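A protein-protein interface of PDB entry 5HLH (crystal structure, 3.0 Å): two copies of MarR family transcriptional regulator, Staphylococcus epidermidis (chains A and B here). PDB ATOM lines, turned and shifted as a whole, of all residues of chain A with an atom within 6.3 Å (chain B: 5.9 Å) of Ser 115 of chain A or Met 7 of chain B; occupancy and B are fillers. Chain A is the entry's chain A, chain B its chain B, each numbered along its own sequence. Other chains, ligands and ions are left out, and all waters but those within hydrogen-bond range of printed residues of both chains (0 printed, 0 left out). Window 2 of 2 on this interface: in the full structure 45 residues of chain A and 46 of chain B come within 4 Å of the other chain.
The side-chain hydroxyl (OH) of Tyr 28 of chain A sits at hydrogen-bond distance from the backbone carbonyl oxygen (O) of Ala 10 of chain B, 3.1 Å away.
The side-chain amide oxygen (OD1) of Asn 11 of chain B sits at hydrogen-bond distance from the side-chain hydroxyl (OH) of Tyr 42 of chain A, at 2.7 Å.
The side-chain amino group (NZ) of Lys 3 of chain B lies within hydrogen-bond range of the backbone carbonyl oxygen (O) of Ser 115 of chain A (3.2 Å).
The backbone NH of Ser 115 of chain A is in hydrogen-bond range of the side-chain sulfur of Met 7 of chain B, 3.7 Å away.
The backbone carbonyl oxygen (O) of Phe 111 of chain A is in hydrogen-bond range of the side-chain hydroxyl (OG) of Ser 115 of chain A (2.7 Å).
The side-chain hydroxyl (OG) of Ser 115 of chain A is in hydrogen-bond range of the backbone carbonyl oxygen (O) of Glu 112 of chain A (2.9 Å).
O of Glu 112 of chain A lies within hydrogen-bond range of OG of Ser 116 of chain A (2.9 Å).
The backbone carbonyl oxygen (O) of Ala 113 of chain A sits at hydrogen-bond distance from the side-chain hydroxyl (OG) of Ser 116 of chain A, 3.4 Å away.
O of Met 7 of chain B sits at hydrogen-bond distance from ND2 of Asn 11 of chain B (2.9 Å).
ND2 of Asn 11 of chain B touches OH of Tyr 28 of chain A, 3.5 Å away.
OH of Tyr 42 of chain A touches CE of Met 7 of chain B, at 3.7 Å.
Asn 11 of chain B touches Leu 46 of chain A.
Phe 111 of chain A touches Met 7 of chain B.
Ile 114 of chain A touches Met 7 of chain B.
Gln 6 of chain B touches Ser 115 of chain A.
Lys 3 of chain B touches Ser 116 of chain A.
Printed residues of chain B within 4 Å of Leu 46 of chain A: Asn 11.
Of the printed residues of chain B, Phe 111 of chain A touches Met 7 (3.3 Å).
Ser 115 of chain A touches just these residues of chain B: Lys 3, Gln 6 and Met 7.
Of the printed residues of chain B, Ser 116 of chain A touches Lys 3 (3.8 Å).
Of chain A, only Tyr 42 (3.7 Å), Phe 111 (3.3 Å), Ile 114 (3.6 Å) and Ser 115 (3.5 Å) come within 4 Å of Met 7 of chain B.
Of the printed residues of chain A, Ala 10 of chain B touches Tyr 28 (3.1 Å).
The nearest printed residue of chain A that does not touch Asn 11 of chain B is Phe 111 of chain A (4.4 Å).
Hydrophobic or aromatic side chains of chain A that line the printed part of chain B: Tyr 28, Tyr 42, Leu 46, Phe 111 and Ile 114.
Among the printed residues, no Asp or Glu carboxylate lies within 4 Å of a Lys or Arg side-chain nitrogen of the other chain.
No position is printed for both chains.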
ATOM      1  N   TYR A  28      14.324   1.947 -13.548  1.00  0.00           N
ATOM      2  CA  TYR A  28      13.031   1.746 -12.927  1.00  0.00           C
ATOM      3  C   TYR A  28      12.591   0.270 -12.948  1.00  0.00           C
ATOM      4  O   TYR A  28      12.095  -0.197 -11.940  1.00  0.00           O
ATOM      5  CB  TYR A  28      11.963   2.671 -13.545  1.00  0.00           C
ATOM      6  CG  TYR A  28      11.972   4.078 -12.972  1.00  0.00           C
ATOM      7  CD1 TYR A  28      12.955   4.990 -13.338  1.00  0.00           C
ATOM      8  CD2 TYR A  28      10.997   4.496 -12.049  1.00  0.00           C
ATOM      9  CE1 TYR A  28      12.982   6.271 -12.820  1.00  0.00           C
ATOM     10  CE2 TYR A  28      11.023   5.785 -11.514  1.00  0.00           C
ATOM     11  CZ  TYR A  28      12.026   6.663 -11.914  1.00  0.00           C
ATOM     12  OH  TYR A  28      12.104   7.947 -11.437  1.00  0.00           O
ATOM     13  N   TYR A  42       3.860   1.863 -14.220  1.00  0.00           N
ATOM     14  CA  TYR A  42       4.219   2.753 -13.126  1.00  0.00           C
ATOM     15  C   TYR A  42       3.797   4.181 -13.445  1.00  0.00           C
ATOM     16  O   TYR A  42       3.233   4.841 -12.599  1.00  0.00           O
ATOM     17  CB  TYR A  42       5.715   2.634 -12.805  1.00  0.00           C
ATOM     18  CG  TYR A  42       6.270   3.649 -11.842  1.00  0.00           C
ATOM     19  CD1 TYR A  42       6.108   3.508 -10.456  1.00  0.00           C
ATOM     20  CD2 TYR A  42       7.000   4.750 -12.314  1.00  0.00           C
ATOM     21  CE1 TYR A  42       6.641   4.453  -9.569  1.00  0.00           C
ATOM     22  CE2 TYR A  42       7.540   5.696 -11.447  1.00  0.00           C
ATOM     23  CZ  TYR A  42       7.362   5.556 -10.080  1.00  0.00           C
ATOM     24  OH  TYR A  42       7.927   6.531  -9.277  1.00  0.00           O
ATOM     25  N   LEU A  46       1.374   6.534 -11.373  1.00  0.00           N
ATOM     26  CA  LEU A  46       1.684   7.875 -10.899  1.00  0.00           C
ATOM     27  C   LEU A  46       0.554   8.880 -11.125  1.00  0.00           C
ATOM     28  O   LEU A  46       0.354   9.766 -10.281  1.00  0.00           O
ATOM     29  CB  LEU A  46       2.924   8.436 -11.568  1.00  0.00           C
ATOM     30  CG  LEU A  46       4.273   7.849 -11.193  1.00  0.00           C
ATOM     31  CD1 LEU A  46       5.299   8.551 -12.065  1.00  0.00           C
ATOM     32  CD2 LEU A  46       4.593   8.018  -9.716  1.00  0.00           C
ATOM     33  N   VAL A 110       6.336   1.235  -2.926  1.00  0.00           N
ATOM     34  CA  VAL A 110       6.909   1.436  -4.268  1.00  0.00           C
ATOM     35  C   VAL A 110       7.870   2.610  -4.260  1.00  0.00           C
ATOM     36  O   VAL A 110       8.999   2.475  -4.728  1.00  0.00           O
ATOM     37  CB  VAL A 110       5.808   1.659  -5.346  1.00  0.00           C
ATOM     38  CG1 VAL A 110       6.364   2.229  -6.649  1.00  0.00           C
ATOM     39  CG2 VAL A 110       5.083   0.351  -5.630  1.00  0.00           C
ATOM     40  N   PHE A 111       7.423   3.747  -3.730  1.00  0.00           N
ATOM     41  CA  PHE A 111       8.255   4.965  -3.695  1.00  0.00           C
ATOM     42  C   PHE A 111       9.554   4.796  -2.877  1.00  0.00           C
ATOM     43  O   PHE A 111      10.605   5.345  -3.249  1.00  0.00           O
ATOM     44  CB  PHE A 111       7.454   6.177  -3.176  1.00  0.00           C
ATOM     45  CG  PHE A 111       6.748   6.968  -4.261  1.00  0.00           C
ATOM     46  CD1 PHE A 111       5.904   6.336  -5.181  1.00  0.00           C
ATOM     47  CD2 PHE A 111       6.913   8.366  -4.355  1.00  0.00           C
ATOM     48  CE1 PHE A 111       5.256   7.072  -6.175  1.00  0.00           C
ATOM     49  CE2 PHE A 111       6.262   9.100  -5.343  1.00  0.00           C
ATOM     50  CZ  PHE A 111       5.435   8.453  -6.256  1.00  0.00           C
ATOM     51  N   GLU A 112       9.474   4.043  -1.774  1.00  0.00           N
ATOM     52  CA  GLU A 112      10.663   3.724  -0.959  1.00  0.00           C
ATOM     53  C   GLU A 112      11.711   2.883  -1.724  1.00  0.00           C
ATOM     54  O   GLU A 112      12.913   3.192  -1.682  1.00  0.00           O
ATOM     55  CB  GLU A 112      10.269   3.013   0.351  1.00  0.00           C
ATOM     56  CG  GLU A 112      11.393   2.974   1.405  1.00  0.00           C
ATOM     57  CD  GLU A 112      10.913   2.721   2.849  1.00  0.00           C
ATOM     58  OE1 GLU A 112       9.682   2.770   3.117  1.00  0.00           O
ATOM     59  OE2 GLU A 112      11.774   2.475   3.737  1.00  0.00           O
ATOM     60  N   ALA A 113      11.237   1.836  -2.411  1.00  0.00           N
ATOM     61  CA  ALA A 113      12.086   0.934  -3.200  1.00  0.00           C
ATOM     62  C   ALA A 113      12.901   1.694  -4.250  1.00  0.00           C
ATOM     63  O   ALA A 113      14.089   1.402  -4.459  1.00  0.00           O
ATOM     64  CB  ALA A 113      11.229  -0.129  -3.866  1.00  0.00           C
ATOM     65  N   ILE A 114      12.263   2.690  -4.868  1.00  0.00           N
ATOM     66  CA  ILE A 114      12.886   3.484  -5.918  1.00  0.00           C
ATOM     67  C   ILE A 114      13.815   4.510  -5.297  1.00  0.00           C
ATOM     68  O   ILE A 114      14.960   4.641  -5.717  1.00  0.00           O
ATOM     69  CB  ILE A 114      11.851   4.259  -6.762  1.00  0.00           C
ATOM     70  CG1 ILE A 114      10.739   3.331  -7.290  1.00  0.00           C
ATOM     71  CG2 ILE A 114      12.545   5.023  -7.899  1.00  0.00           C
ATOM     72  CD1 ILE A 114      10.961   2.730  -8.659  1.00  0.00           C
ATOM     73  N   SER A 115      13.299   5.253  -4.319  1.00  0.00           N
ATOM     74  CA  SER A 115      14.021   6.384  -3.679  1.00  0.00           C
ATOM     75  C   SER A 115      15.351   5.972  -3.015  1.00  0.00           C
ATOM     76  O   SER A 115      16.358   6.689  -3.110  1.00  0.00           O
ATOM     77  CB  SER A 115      13.121   7.042  -2.631  1.00  0.00           C
ATOM     78  OG  SER A 115      12.687   6.055  -1.699  1.00  0.00           O
ATOM     79  N   SER A 116      15.356   4.800  -2.374  1.00  0.00           N
ATOM     80  CA  SER A 116      16.559   4.267  -1.700  1.00  0.00           C
ATOM     81  C   SER A 116      17.716   3.848  -2.651  1.00  0.00           C
ATOM     82  O   SER A 116      18.745   3.334  -2.190  1.00  0.00           O
ATOM     83  CB  SER A 116      16.170   3.088  -0.767  1.00  0.00           C
ATOM     84  OG  SER A 116      15.544   2.013  -1.479  1.00  0.00           O
ATOM     85  N   CYS A 117      17.555   4.052  -3.958  1.00  0.00           N
ATOM     86  CA  CYS A 117      18.612   3.777  -4.917  1.00  0.00           C
ATOM     87  C   CYS A 117      18.916   5.020  -5.731  1.00  0.00           C
ATOM     88  O   CYS A 117      19.791   4.970  -6.591  1.00  0.00           O
ATOM     89  CB  CYS A 117      18.219   2.594  -5.822  1.00  0.00           C
ATOM     90  SG  CYS A 117      18.255   1.002  -4.950  1.00  0.00           S
ATOM     91  N   LYS B   3      13.226  13.351   1.263  1.00  0.00           N
ATOM     92  CA  LYS B   3      13.469  12.334   0.243  1.00  0.00           C
ATOM     93  C   LYS B   3      12.397  12.399  -0.871  1.00  0.00           C
ATOM     94  O   LYS B   3      12.701  12.195  -2.051  1.00  0.00           O
ATOM     95  CB  LYS B   3      13.493  10.939   0.897  1.00  0.00           C
ATOM     96  CG  LYS B   3      14.413   9.938   0.212  1.00  0.00           C
ATOM     97  CD  LYS B   3      14.218   8.529   0.768  1.00  0.00           C
ATOM     98  CE  LYS B   3      15.543   7.822   1.077  1.00  0.00           C
ATOM     99  NZ  LYS B   3      16.474   7.666  -0.078  1.00  0.00           N
ATOM    100  N   GLN B   4      11.154  12.704  -0.471  1.00  0.00           N
ATOM    101  CA  GLN B   4       9.996  12.799  -1.380  1.00  0.00           C
ATOM    102  C   GLN B   4      10.166  13.823  -2.515  1.00  0.00           C
ATOM    103  O   GLN B   4       9.602  13.649  -3.604  1.00  0.00           O
ATOM    104  CB  GLN B   4       8.733  13.149  -0.578  1.00  0.00           C
ATOM    105  CG  GLN B   4       7.443  13.117  -1.387  1.00  0.00           C
ATOM    106  CD  GLN B   4       6.211  13.204  -0.509  1.00  0.00           C
ATOM    107  OE1 GLN B   4       6.228  13.849   0.544  1.00  0.00           O
ATOM    108  NE2 GLN B   4       5.131  12.550  -0.935  1.00  0.00           N
ATOM    109  N   GLU B   5      10.910  14.894  -2.242  1.00  0.00           N
ATOM    110  CA  GLU B   5      11.157  15.959  -3.229  1.00  0.00           C
ATOM    111  C   GLU B   5      12.155  15.532  -4.297  1.00  0.00           C
ATOM    112  O   GLU B   5      12.083  15.996  -5.447  1.00  0.00           O
ATOM    113  CB  GLU B   5      11.697  17.219  -2.546  1.00  0.00           C
ATOM    114  CG  GLU B   5      11.483  18.489  -3.364  1.00  0.00           C
ATOM    115  CD  GLU B   5      10.093  19.081  -3.190  1.00  0.00           C
ATOM    116  OE1 GLU B   5       9.348  18.655  -2.273  1.00  0.00           O
ATOM    117  OE2 GLU B   5       9.742  19.982  -3.982  1.00  0.00           O
ATOM    118  N   GLN B   6      13.100  14.681  -3.887  1.00  0.00           N
ATOM    119  CA  GLN B   6      14.098  14.123  -4.800  1.00  0.00           C
ATOM    120  C   GLN B   6      13.417  13.110  -5.751  1.00  0.00           C
ATOM    121  O   GLN B   6      13.725  13.092  -6.950  1.00  0.00           O
ATOM    122  CB  GLN B   6      15.311  13.538  -4.025  1.00  0.00           C
ATOM    123  CG  GLN B   6      15.302  12.032  -3.759  1.00  0.00           C
ATOM    124  CD  GLN B   6      16.202  11.592  -2.616  1.00  0.00           C
ATOM    125  OE1 GLN B   6      16.644  12.401  -1.798  1.00  0.00           O
ATOM    126  NE2 GLN B   6      16.466  10.288  -2.550  1.00  0.00           N
ATOM    127  N   MET B   7      12.473  12.313  -5.227  1.00  0.00           N
ATOM    128  CA  MET B   7      11.666  11.402  -6.061  1.00  0.00           C
ATOM    129  C   MET B   7      10.839  12.137  -7.120  1.00  0.00           C
ATOM    130  O   MET B   7      10.822  11.751  -8.291  1.00  0.00           O
ATOM    131  CB  MET B   7      10.743  10.535  -5.206  1.00  0.00           C
ATOM    132  CG  MET B   7      11.359   9.205  -4.801  1.00  0.00           C
ATOM    133  SD  MET B   7      11.366   7.904  -6.063  1.00  0.00           S
ATOM    134  CE  MET B   7       9.607   7.543  -6.165  1.00  0.00           C
ATOM    135  N   ARG B   8      10.172  13.209  -6.725  1.00  0.00           N
ATOM    136  CA  ARG B   8       9.371  13.966  -7.682  1.00  0.00           C
ATOM    137  C   ARG B   8      10.254  14.469  -8.854  1.00  0.00           C
ATOM    138  O   ARG B   8       9.788  14.531  -9.996  1.00  0.00           O
ATOM    139  CB  ARG B   8       8.619  15.117  -6.983  1.00  0.00           C
ATOM    140  CG  ARG B   8       7.233  15.403  -7.564  1.00  0.00           C
ATOM    141  CD  ARG B   8       6.576  16.624  -6.925  1.00  0.00           C
ATOM    142  NE  ARG B   8       6.947  17.870  -7.623  1.00  0.00           N
ATOM    143  CZ  ARG B   8       7.482  18.974  -7.076  1.00  0.00           C
ATOM    144  NH1 ARG B   8       7.725  19.080  -5.765  1.00  0.00           N
ATOM    145  NH2 ARG B   8       7.769  20.010  -7.866  1.00  0.00           N
ATOM    146  N   LEU B   9      11.521  14.786  -8.557  1.00  0.00           N
ATOM    147  CA  LEU B   9      12.496  15.255  -9.549  1.00  0.00           C
ATOM    148  C   LEU B   9      12.903  14.154 -10.516  1.00  0.00           C
ATOM    149  O   LEU B   9      12.930  14.365 -11.732  1.00  0.00           O
ATOM    150  CB  LEU B   9      13.741  15.805  -8.837  1.00  0.00           C
ATOM    151  CG  LEU B   9      14.851  16.527  -9.621  1.00  0.00           C
ATOM    152  CD1 LEU B   9      15.915  15.560 -10.141  1.00  0.00           C
ATOM    153  CD2 LEU B   9      14.312  17.411 -10.746  1.00  0.00           C
ATOM    154  N   ALA B  10      13.230  12.985  -9.968  1.00  0.00           N
ATOM    155  CA  ALA B  10      13.513  11.783 -10.771  1.00  0.00           C
ATOM    156  C   ALA B  10      12.314  11.294 -11.602  1.00  0.00           C
ATOM    157  O   ALA B  10      12.513  10.718 -12.684  1.00  0.00           O
ATOM    158  CB  ALA B  10      13.993  10.653  -9.876  1.00  0.00           C
ATOM    159  N   ASN B  11      11.089  11.513 -11.103  1.00  0.00           N
ATOM    160  CA  ASN B  11       9.865  11.096 -11.810  1.00  0.00           C
ATOM    161  C   ASN B  11       9.584  12.007 -12.987  1.00  0.00           C
ATOM    162  O   ASN B  11       9.280  11.528 -14.071  1.00  0.00           O
ATOM    163  CB  ASN B  11       8.640  11.040 -10.887  1.00  0.00           C
ATOM    164  CG  ASN B  11       8.555   9.750 -10.095  1.00  0.00           C
ATOM    165  OD1 ASN B  11       7.531   9.092 -10.084  1.00  0.00           O
ATOM    166  ND2 ASN B  11       9.628   9.393  -9.417  1.00  0.00           N
ATOM    167  N   GLN B  12       9.715  13.316 -12.789  1.00  0.00           N
ATOM    168  CA  GLN B  12       9.567  14.259 -13.898  1.00  0.00           C
ATOM    169  C   GLN B  12      10.824  14.388 -14.783  1.00  0.00           C
ATOM    170  O   GLN B  12      10.900  15.285 -15.627  1.00  0.00           O
ATOM    171  CB  GLN B  12       9.026  15.631 -13.422  1.00  0.00           C
ATOM    172  CG  GLN B  12       9.991  16.547 -12.671  1.00  0.00           C
ATOM    173  CD  GLN B  12       9.288  17.785 -12.082  1.00  0.00           C
ATOM    174  OE1 GLN B  12       8.726  18.605 -12.821  1.00  0.00           O
ATOM    175  NE2 GLN B  12       9.327  17.926 -10.750  1.00  0.00           N
